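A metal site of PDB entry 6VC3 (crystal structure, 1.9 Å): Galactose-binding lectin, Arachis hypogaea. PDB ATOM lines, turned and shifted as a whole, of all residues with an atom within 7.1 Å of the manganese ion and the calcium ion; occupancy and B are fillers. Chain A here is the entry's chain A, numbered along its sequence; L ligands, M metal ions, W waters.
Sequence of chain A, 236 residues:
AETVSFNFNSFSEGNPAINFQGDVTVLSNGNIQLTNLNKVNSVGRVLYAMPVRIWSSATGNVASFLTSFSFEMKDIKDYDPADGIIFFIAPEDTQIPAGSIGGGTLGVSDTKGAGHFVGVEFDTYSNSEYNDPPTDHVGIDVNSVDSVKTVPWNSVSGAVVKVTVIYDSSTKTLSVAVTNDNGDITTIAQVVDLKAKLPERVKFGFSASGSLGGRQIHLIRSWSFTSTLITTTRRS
The side-chain amide nitrogen (ND2) of Asn 127 is in hydrogen-bond range of an oxygen (O3) of the ligand, at 2.9 Å.
OD1 of Asp 83 lies within hydrogen-bond range of O4 of the ligand, 2.6 Å away.
The backbone NH (N) of Gly 104 is in hydrogen-bond range of an oxygen (O3) of the ligand.
ND1 of His 137 is in hydrogen-bond range of O of Thr 135, at 2.9 Å.
OG of Ser 147 lies close to OE2 of Glu 121 (3.5 Å).
The backbone carbonyl oxygen (O) of Gly 139 is in hydrogen-bond range of the backbone NH (N) of Glu 121.
The manganese ion is bound by OD2 of Asp 123 (2.1 Å), water W4 (2.1 Å), OD1 of Asp 132 (2.1 Å), NE2 of His 137 (2.2 Å), water W2 (2.2 Å) and OE2 of Glu 121 (2.3 Å).
The calcium ion is bound by O of Tyr 125, water W1, water W3, OD2 of Asp 132, OD1 of Asn 127, OD1 of Asp 123 and OD2 of Asp 123.
The calcium ion has seven donor atoms within binding distance.
Water W4 bridges the side-chain carboxylate of Glu 121 (2.7 Å) and the backbone carbonyl oxygen of Val 145 (2.7 Å).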
ATOM      1  N   ASP A  83      21.882  10.219   5.601  1.00  0.00           N
ATOM      2  CA  ASP A  83      20.470  10.036   5.921  1.00  0.00           C
ATOM      3  C   ASP A  83      19.640  11.307   6.056  1.00  0.00           C
ATOM      4  O   ASP A  83      18.396  11.233   5.982  1.00  0.00           O
ATOM      5  CB  ASP A  83      20.372   9.217   7.204  1.00  0.00           C
ATOM      6  CG  ASP A  83      20.357   7.728   6.946  1.00  0.00           C
ATOM      7  OD1 ASP A  83      21.477   7.112   6.816  1.00  0.00           O
ATOM      8  OD2 ASP A  83      19.247   7.156   6.904  1.00  0.00           O
ATOM      9  N   GLY A  84      20.305  12.445   6.232  1.00  0.00           N
ATOM     10  CA  GLY A  84      19.662  13.736   6.361  1.00  0.00           C
ATOM     11  C   GLY A  84      20.112  14.538   7.550  1.00  0.00           C
ATOM     12  O   GLY A  84      20.982  14.113   8.321  1.00  0.00           O
ATOM     13  N   GLY A 103      22.323   6.334  10.983  1.00  0.00           N
ATOM     14  CA  GLY A 103      21.313   6.083   9.952  1.00  0.00           C
ATOM     15  C   GLY A 103      20.024   6.876  10.119  1.00  0.00           C
ATOM     16  O   GLY A 103      20.035   8.114  10.164  1.00  0.00           O
ATOM     17  N   GLY A 104      18.933   6.127  10.252  1.00  0.00           N
ATOM     18  CA  GLY A 104      17.574   6.645  10.380  1.00  0.00           C
ATOM     19  C   GLY A 104      17.269   7.318  11.702  1.00  0.00           C
ATOM     20  O   GLY A 104      16.237   7.989  11.822  1.00  0.00           O
ATOM     21  N   THR A 105      18.148   7.113  12.731  1.00  0.00           N
ATOM     22  CA  THR A 105      17.981   7.741  14.048  1.00  0.00           C
ATOM     23  C   THR A 105      18.217   9.255  13.948  1.00  0.00           C
ATOM     24  O   THR A 105      17.796   9.981  14.838  1.00  0.00           O
ATOM     25  CB  THR A 105      18.931   7.106  15.113  1.00  0.00           C
ATOM     26  OG1 THR A 105      20.290   7.428  14.833  1.00  0.00           O
ATOM     27  CG2 THR A 105      18.752   5.612  15.239  1.00  0.00           C
ATOM     28  N   LEU A 106      18.939   9.703  12.895  1.00  0.00           N
ATOM     29  CA  LEU A 106      19.345  11.089  12.594  1.00  0.00           C
ATOM     30  C   LEU A 106      20.221  11.674  13.735  1.00  0.00           C
ATOM     31  O   LEU A 106      20.293  12.910  13.897  1.00  0.00           O
ATOM     32  CB  LEU A 106      18.132  12.006  12.275  1.00  0.00           C
ATOM     33  CG  LEU A 106      17.275  11.660  11.042  1.00  0.00           C
ATOM     34  CD1 LEU A 106      16.124  12.603  10.915  1.00  0.00           C
ATOM     35  CD2 LEU A 106      18.101  11.640   9.744  1.00  0.00           C
ATOM     36  N   GLU A 121      13.166  17.700  10.785  1.00  0.00           N
ATOM     37  CA  GLU A 121      14.038  16.865   9.991  1.00  0.00           C
ATOM     38  C   GLU A 121      13.895  17.142   8.485  1.00  0.00           C
ATOM     39  O   GLU A 121      12.831  17.569   8.012  1.00  0.00           O
ATOM     40  CB  GLU A 121      13.786  15.374  10.274  1.00  0.00           C
ATOM     41  CG  GLU A 121      12.370  14.917   9.995  1.00  0.00           C
ATOM     42  CD  GLU A 121      12.215  13.417   9.884  1.00  0.00           C
ATOM     43  OE1 GLU A 121      12.589  12.716  10.846  1.00  0.00           O
ATOM     44  OE2 GLU A 121      11.673  12.951   8.858  1.00  0.00           O
ATOM     45  N   PHE A 122      15.005  16.899   7.771  1.00  0.00           N
ATOM     46  CA  PHE A 122      15.172  17.018   6.321  1.00  0.00           C
ATOM     47  C   PHE A 122      15.701  15.661   5.883  1.00  0.00           C
ATOM     48  O   PHE A 122      16.910  15.453   5.702  1.00  0.00           O
ATOM     49  CB  PHE A 122      16.101  18.199   5.978  1.00  0.00           C
ATOM     50  CG  PHE A 122      15.567  19.522   6.468  1.00  0.00           C
ATOM     51  CD1 PHE A 122      14.724  20.283   5.666  1.00  0.00           C
ATOM     52  CD2 PHE A 122      15.866  19.990   7.748  1.00  0.00           C
ATOM     53  CE1 PHE A 122      14.216  21.508   6.130  1.00  0.00           C
ATOM     54  CE2 PHE A 122      15.340  21.188   8.215  1.00  0.00           C
ATOM     55  CZ  PHE A 122      14.512  21.936   7.403  1.00  0.00           C
ATOM     56  N   ASP A 123      14.774  14.727   5.826  1.00  0.00           N
ATOM     57  CA  ASP A 123      14.979  13.326   5.574  1.00  0.00           C
ATOM     58  C   ASP A 123      15.074  12.991   4.096  1.00  0.00           C
ATOM     59  O   ASP A 123      14.154  13.290   3.328  1.00  0.00           O
ATOM     60  CB  ASP A 123      13.844  12.544   6.233  1.00  0.00           C
ATOM     61  CG  ASP A 123      14.217  11.133   6.580  1.00  0.00           C
ATOM     62  OD1 ASP A 123      15.076  10.561   5.892  1.00  0.00           O
ATOM     63  OD2 ASP A 123      13.681  10.617   7.567  1.00  0.00           O
ATOM     64  N   THR A 124      16.200  12.282   3.733  1.00  0.00           N
ATOM     65  CA  THR A 124      16.589  11.900   2.374  1.00  0.00           C
ATOM     66  C   THR A 124      16.620  10.372   2.138  1.00  0.00           C
ATOM     67  O   THR A 124      17.052   9.941   1.073  1.00  0.00           O
ATOM     68  CB  THR A 124      17.995  12.477   2.063  1.00  0.00           C
ATOM     69  OG1 THR A 124      18.992  11.784   2.802  1.00  0.00           O
ATOM     70  CG2 THR A 124      18.079  13.965   2.315  1.00  0.00           C
ATOM     71  N   TYR A 125      16.113   9.573   3.101  1.00  0.00           N
ATOM     72  CA  TYR A 125      16.045   8.099   2.981  1.00  0.00           C
ATOM     73  C   TYR A 125      14.776   7.577   3.672  1.00  0.00           C
ATOM     74  O   TYR A 125      14.484   7.993   4.795  1.00  0.00           O
ATOM     75  CB  TYR A 125      17.302   7.397   3.543  1.00  0.00           C
ATOM     76  CG  TYR A 125      17.274   5.893   3.361  1.00  0.00           C
ATOM     77  CD1 TYR A 125      16.644   5.070   4.296  1.00  0.00           C
ATOM     78  CD2 TYR A 125      17.818   5.294   2.231  1.00  0.00           C
ATOM     79  CE1 TYR A 125      16.518   3.695   4.078  1.00  0.00           C
ATOM     80  CE2 TYR A 125      17.745   3.916   2.035  1.00  0.00           C
ATOM     81  CZ  TYR A 125      17.091   3.120   2.967  1.00  0.00           C
ATOM     82  OH  TYR A 125      17.003   1.753   2.795  1.00  0.00           O
ATOM     83  N   SER A 126      14.071   6.629   3.020  1.00  0.00           N
ATOM     84  CA  SER A 126      12.834   6.075   3.554  1.00  0.00           C
ATOM     85  C   SER A 126      13.088   4.836   4.420  1.00  0.00           C
ATOM     86  O   SER A 126      13.327   3.736   3.916  1.00  0.00           O
ATOM     87  CB  SER A 126      11.836   5.753   2.438  1.00  0.00           C
ATOM     88  OG  SER A 126      10.563   5.451   2.968  1.00  0.00           O
ATOM     89  N   ASN A 127      13.008   5.037   5.744  1.00  0.00           N
ATOM     90  CA  ASN A 127      13.157   4.039   6.797  1.00  0.00           C
ATOM     91  C   ASN A 127      11.789   3.490   7.208  1.00  0.00           C
ATOM     92  O   ASN A 127      11.073   4.148   7.957  1.00  0.00           O
ATOM     93  CB  ASN A 127      13.896   4.639   8.011  1.00  0.00           C
ATOM     94  CG  ASN A 127      15.340   4.971   7.741  1.00  0.00           C
ATOM     95  OD1 ASN A 127      15.668   6.077   7.322  1.00  0.00           O
ATOM     96  ND2 ASN A 127      16.222   4.004   7.952  1.00  0.00           N
ATOM     97  N   SER A 128      11.441   2.261   6.740  1.00  0.00           N
ATOM     98  CA  SER A 128      10.147   1.626   7.034  1.00  0.00           C
ATOM     99  C   SER A 128       9.963   1.368   8.515  1.00  0.00           C
ATOM    100  O   SER A 128       8.836   1.435   9.010  1.00  0.00           O
ATOM    101  CB  SER A 128       9.974   0.334   6.235  1.00  0.00           C
ATOM    102  OG  SER A 128      11.034  -0.576   6.466  1.00  0.00           O
ATOM    103  N   TYR A 130      10.693   3.321  10.896  1.00  0.00           N
ATOM    104  CA  TYR A 130      10.240   4.568  11.539  1.00  0.00           C
ATOM    105  C   TYR A 130       9.034   5.162  10.792  1.00  0.00           C
ATOM    106  O   TYR A 130       8.716   6.340  10.978  1.00  0.00           O
ATOM    107  CB  TYR A 130      11.388   5.594  11.653  1.00  0.00           C
ATOM    108  CG  TYR A 130      12.652   5.008  12.266  1.00  0.00           C
ATOM    109  CD1 TYR A 130      12.615   4.345  13.486  1.00  0.00           C
ATOM    110  CD2 TYR A 130      13.883   5.142  11.624  1.00  0.00           C
ATOM    111  CE1 TYR A 130      13.766   3.791  14.038  1.00  0.00           C
ATOM    112  CE2 TYR A 130      15.032   4.605  12.179  1.00  0.00           C
ATOM    113  CZ  TYR A 130      14.983   3.942  13.392  1.00  0.00           C
ATOM    114  OH  TYR A 130      16.118   3.422  13.942  1.00  0.00           O
ATOM    115  N   ASN A 131       8.344   4.335   9.976  1.00  0.00           N
ATOM    116  CA  ASN A 131       7.176   4.665   9.151  1.00  0.00           C
ATOM    117  C   ASN A 131       7.370   5.958   8.325  1.00  0.00           C
ATOM    118  O   ASN A 131       6.500   6.827   8.299  1.00  0.00           O
ATOM    119  CB  ASN A 131       5.890   4.726  10.008  1.00  0.00           C
ATOM    120  CG  ASN A 131       5.446   3.393  10.541  1.00  0.00           C
ATOM    121  OD1 ASN A 131       5.275   2.415   9.808  1.00  0.00           O
ATOM    122  ND2 ASN A 131       5.218   3.340  11.844  1.00  0.00           N
ATOM    123  N   ASP A 132       8.528   6.058   7.654  1.00  0.00           N
ATOM    124  CA  ASP A 132       8.864   7.187   6.794  1.00  0.00           C
ATOM    125  C   ASP A 132       7.977   7.238   5.541  1.00  0.00           C
ATOM    126  O   ASP A 132       7.723   6.185   4.957  1.00  0.00           O
ATOM    127  CB  ASP A 132      10.334   7.098   6.323  1.00  0.00           C
ATOM    128  CG  ASP A 132      11.364   7.796   7.187  1.00  0.00           C
ATOM    129  OD1 ASP A 132      11.000   8.730   7.923  1.00  0.00           O
ATOM    130  OD2 ASP A 132      12.561   7.470   7.055  1.00  0.00           O
ATOM    131  N   PRO A 133       7.577   8.427   5.029  1.00  0.00           N
ATOM    132  CA  PRO A 133       6.829   8.464   3.755  1.00  0.00           C
ATOM    133  C   PRO A 133       7.710   7.934   2.601  1.00  0.00           C
ATOM    134  O   PRO A 133       8.926   7.805   2.795  1.00  0.00           O
ATOM    135  CB  PRO A 133       6.443   9.939   3.600  1.00  0.00           C
ATOM    136  CG  PRO A 133       7.351  10.677   4.483  1.00  0.00           C
ATOM    137  CD  PRO A 133       7.777   9.786   5.583  1.00  0.00           C
ATOM    138  N   THR A 135       8.947   9.186  -0.270  1.00  0.00           N
ATOM    139  CA  THR A 135       9.915  10.098  -0.893  1.00  0.00           C
ATOM    140  C   THR A 135      10.630  10.970   0.147  1.00  0.00           C
ATOM    141  O   THR A 135      10.245  10.936   1.328  1.00  0.00           O
ATOM    142  CB  THR A 135       9.212  11.010  -1.924  1.00  0.00           C
ATOM    143  OG1 THR A 135       8.328  11.915  -1.260  1.00  0.00           O
ATOM    144  CG2 THR A 135       8.474  10.233  -3.012  1.00  0.00           C
ATOM    145  N   HIS A 137      11.497  14.118   2.482  1.00  0.00           N
ATOM    146  CA  HIS A 137      10.506  14.901   3.214  1.00  0.00           C
ATOM    147  C   HIS A 137      11.046  15.774   4.309  1.00  0.00           C
ATOM    148  O   HIS A 137      12.123  15.571   4.861  1.00  0.00           O
ATOM    149  CB  HIS A 137       9.441  13.974   3.847  1.00  0.00           C
ATOM    150  CG  HIS A 137      10.027  12.884   4.697  1.00  0.00           C
ATOM    151  ND1 HIS A 137      10.538  11.737   4.132  1.00  0.00           N
ATOM    152  CD2 HIS A 137      10.174  12.816   6.040  1.00  0.00           C
ATOM    153  CE1 HIS A 137      10.940  10.995   5.145  1.00  0.00           C
ATOM    154  NE2 HIS A 137      10.736  11.606   6.306  1.00  0.00           N
ATOM    155  N   VAL A 138      10.207  16.755   4.657  1.00  0.00           N
ATOM    156  CA  VAL A 138      10.425  17.611   5.800  1.00  0.00           C
ATOM    157  C   VAL A 138       9.448  17.071   6.838  1.00  0.00           C
ATOM    158  O   VAL A 138       8.316  16.737   6.487  1.00  0.00           O
ATOM    159  CB  VAL A 138      10.277  19.114   5.475  1.00  0.00           C
ATOM    160  CG1 VAL A 138      10.486  19.972   6.726  1.00  0.00           C
ATOM    161  CG2 VAL A 138      11.261  19.521   4.390  1.00  0.00           C
ATOM    162  N   GLY A 139       9.924  16.836   8.048  1.00  0.00           N
ATOM    163  CA  GLY A 139       9.112  16.262   9.105  1.00  0.00           C
ATOM    164  C   GLY A 139       9.237  17.023  10.402  1.00  0.00           C
ATOM    165  O   GLY A 139      10.245  17.677  10.659  1.00  0.00           O
ATOM    166  N   ASP A 141       9.068  16.403  14.398  1.00  0.00           N
ATOM    167  CA  ASP A 141       9.369  15.297  15.319  1.00  0.00           C
ATOM    168  C   ASP A 141       9.189  15.685  16.770  1.00  0.00           C
ATOM    169  O   ASP A 141       9.655  16.750  17.187  1.00  0.00           O
ATOM    170  CB  ASP A 141      10.833  14.846  15.097  1.00  0.00           C
ATOM    171  CG  ASP A 141      11.108  14.163  13.773  1.00  0.00           C
ATOM    172  OD1 ASP A 141      10.177  14.134  12.915  1.00  0.00           O
ATOM    173  OD2 ASP A 141      12.251  13.637  13.589  1.00  0.00           O
ATOM    174  N   VAL A 145      11.670   9.824  15.740  1.00  0.00           N
ATOM    175  CA  VAL A 145      11.991  10.023  14.323  1.00  0.00           C
ATOM    176  C   VAL A 145      10.814   9.467  13.476  1.00  0.00           C
ATOM    177  O   VAL A 145      10.822   9.536  12.244  1.00  0.00           O
ATOM    178  CB  VAL A 145      13.377   9.501  13.856  1.00  0.00           C
ATOM    179  CG1 VAL A 145      14.504  10.390  14.369  1.00  0.00           C
ATOM    180  CG2 VAL A 145      13.611   8.040  14.242  1.00  0.00           C
ATOM    181  N   ASP A 146       9.793   8.918  14.145  1.00  0.00           N
ATOM    182  CA  ASP A 146       8.515   8.562  13.521  1.00  0.00           C
ATOM    183  C   ASP A 146       7.707   9.853  13.661  1.00  0.00           C
ATOM    184  O   ASP A 146       7.121  10.111  14.712  1.00  0.00           O
ATOM    185  CB  ASP A 146       7.856   7.318  14.181  1.00  0.00           C
ATOM    186  CG  ASP A 146       6.619   6.769  13.471  1.00  0.00           C
ATOM    187  OD1 ASP A 146       6.012   7.501  12.654  1.00  0.00           O
ATOM    188  OD2 ASP A 146       6.242   5.613  13.743  1.00  0.00           O
ATOM    189  N   SER A 147       7.823  10.733  12.641  1.00  0.00           N
ATOM    190  CA  SER A 147       7.279  12.088  12.597  1.00  0.00           C
ATOM    191  C   SER A 147       5.799  12.198  12.948  1.00  0.00           C
ATOM    192  O   SER A 147       4.978  11.357  12.530  1.00  0.00           O
ATOM    193  CB  SER A 147       7.488  12.715  11.221  1.00  0.00           C
ATOM    194  OG  SER A 147       8.852  12.978  10.909  1.00  0.00           O
ATOM    195  N   THR A 150       4.547  14.986   8.251  1.00  0.00           N
ATOM    196  CA  THR A 150       5.526  15.113   7.172  1.00  0.00           C
ATOM    197  C   THR A 150       4.925  15.827   5.970  1.00  0.00           C
ATOM    198  O   THR A 150       3.720  15.809   5.778  1.00  0.00           O
ATOM    199  CB  THR A 150       6.086  13.743   6.696  1.00  0.00           C
ATOM    200  OG1 THR A 150       5.009  12.915   6.274  1.00  0.00           O
ATOM    201  CG2 THR A 150       6.974  13.064   7.730  1.00  0.00           C
HETATM  202  C1  LIG L   1      20.059   4.084   5.444  1.00  0.00           C
HETATM  203  C2  LIG L   1      19.237   3.567   6.633  1.00  0.00           C
HETATM  204  C3  LIG L   1      20.361   2.933   4.492  1.00  0.00           C
HETATM  205  C4  LIG L   1      20.266   1.320   6.253  1.00  0.00           C
HETATM  206  C5  LIG L   1      19.942   2.386   7.296  1.00  0.00           C
HETATM  207  C6  LIG L   1      21.232   3.316   3.322  1.00  0.00           C
HETATM  208  O1  LIG L   1      21.040   1.878   5.193  1.00  0.00           O
HETATM  209  O2  LIG L   1      19.143   1.848   8.331  1.00  0.00           O
HETATM  210  O3  LIG L   1      19.012   4.607   7.572  1.00  0.00           O
HETATM  211  O4  LIG L   1      21.281   4.640   5.910  1.00  0.00           O
HETATM  212  O5  LIG L   1      20.946   2.535   2.177  1.00  0.00           O
HETATM  213  S1  LIG L   1      21.113  -0.092   6.991  1.00  0.00           S
HETATM  214 MN    MN M   1      11.683  10.743   8.120  1.00  0.00          MN
HETATM  215 CA    CA M   2      14.724   8.262   6.980  1.00  0.00          CA
HETATM  216  O   HOH W   1      14.695   8.393   9.227  1.00  0.00           O
HETATM  217  O   HOH W   2       9.583  11.134   8.800  1.00  0.00           O
HETATM  218  O   HOH W   3      16.975   8.602   7.167  1.00  0.00           O
HETATM  219  O   HOH W   4      12.303  10.200  10.045  1.00  0.00           O
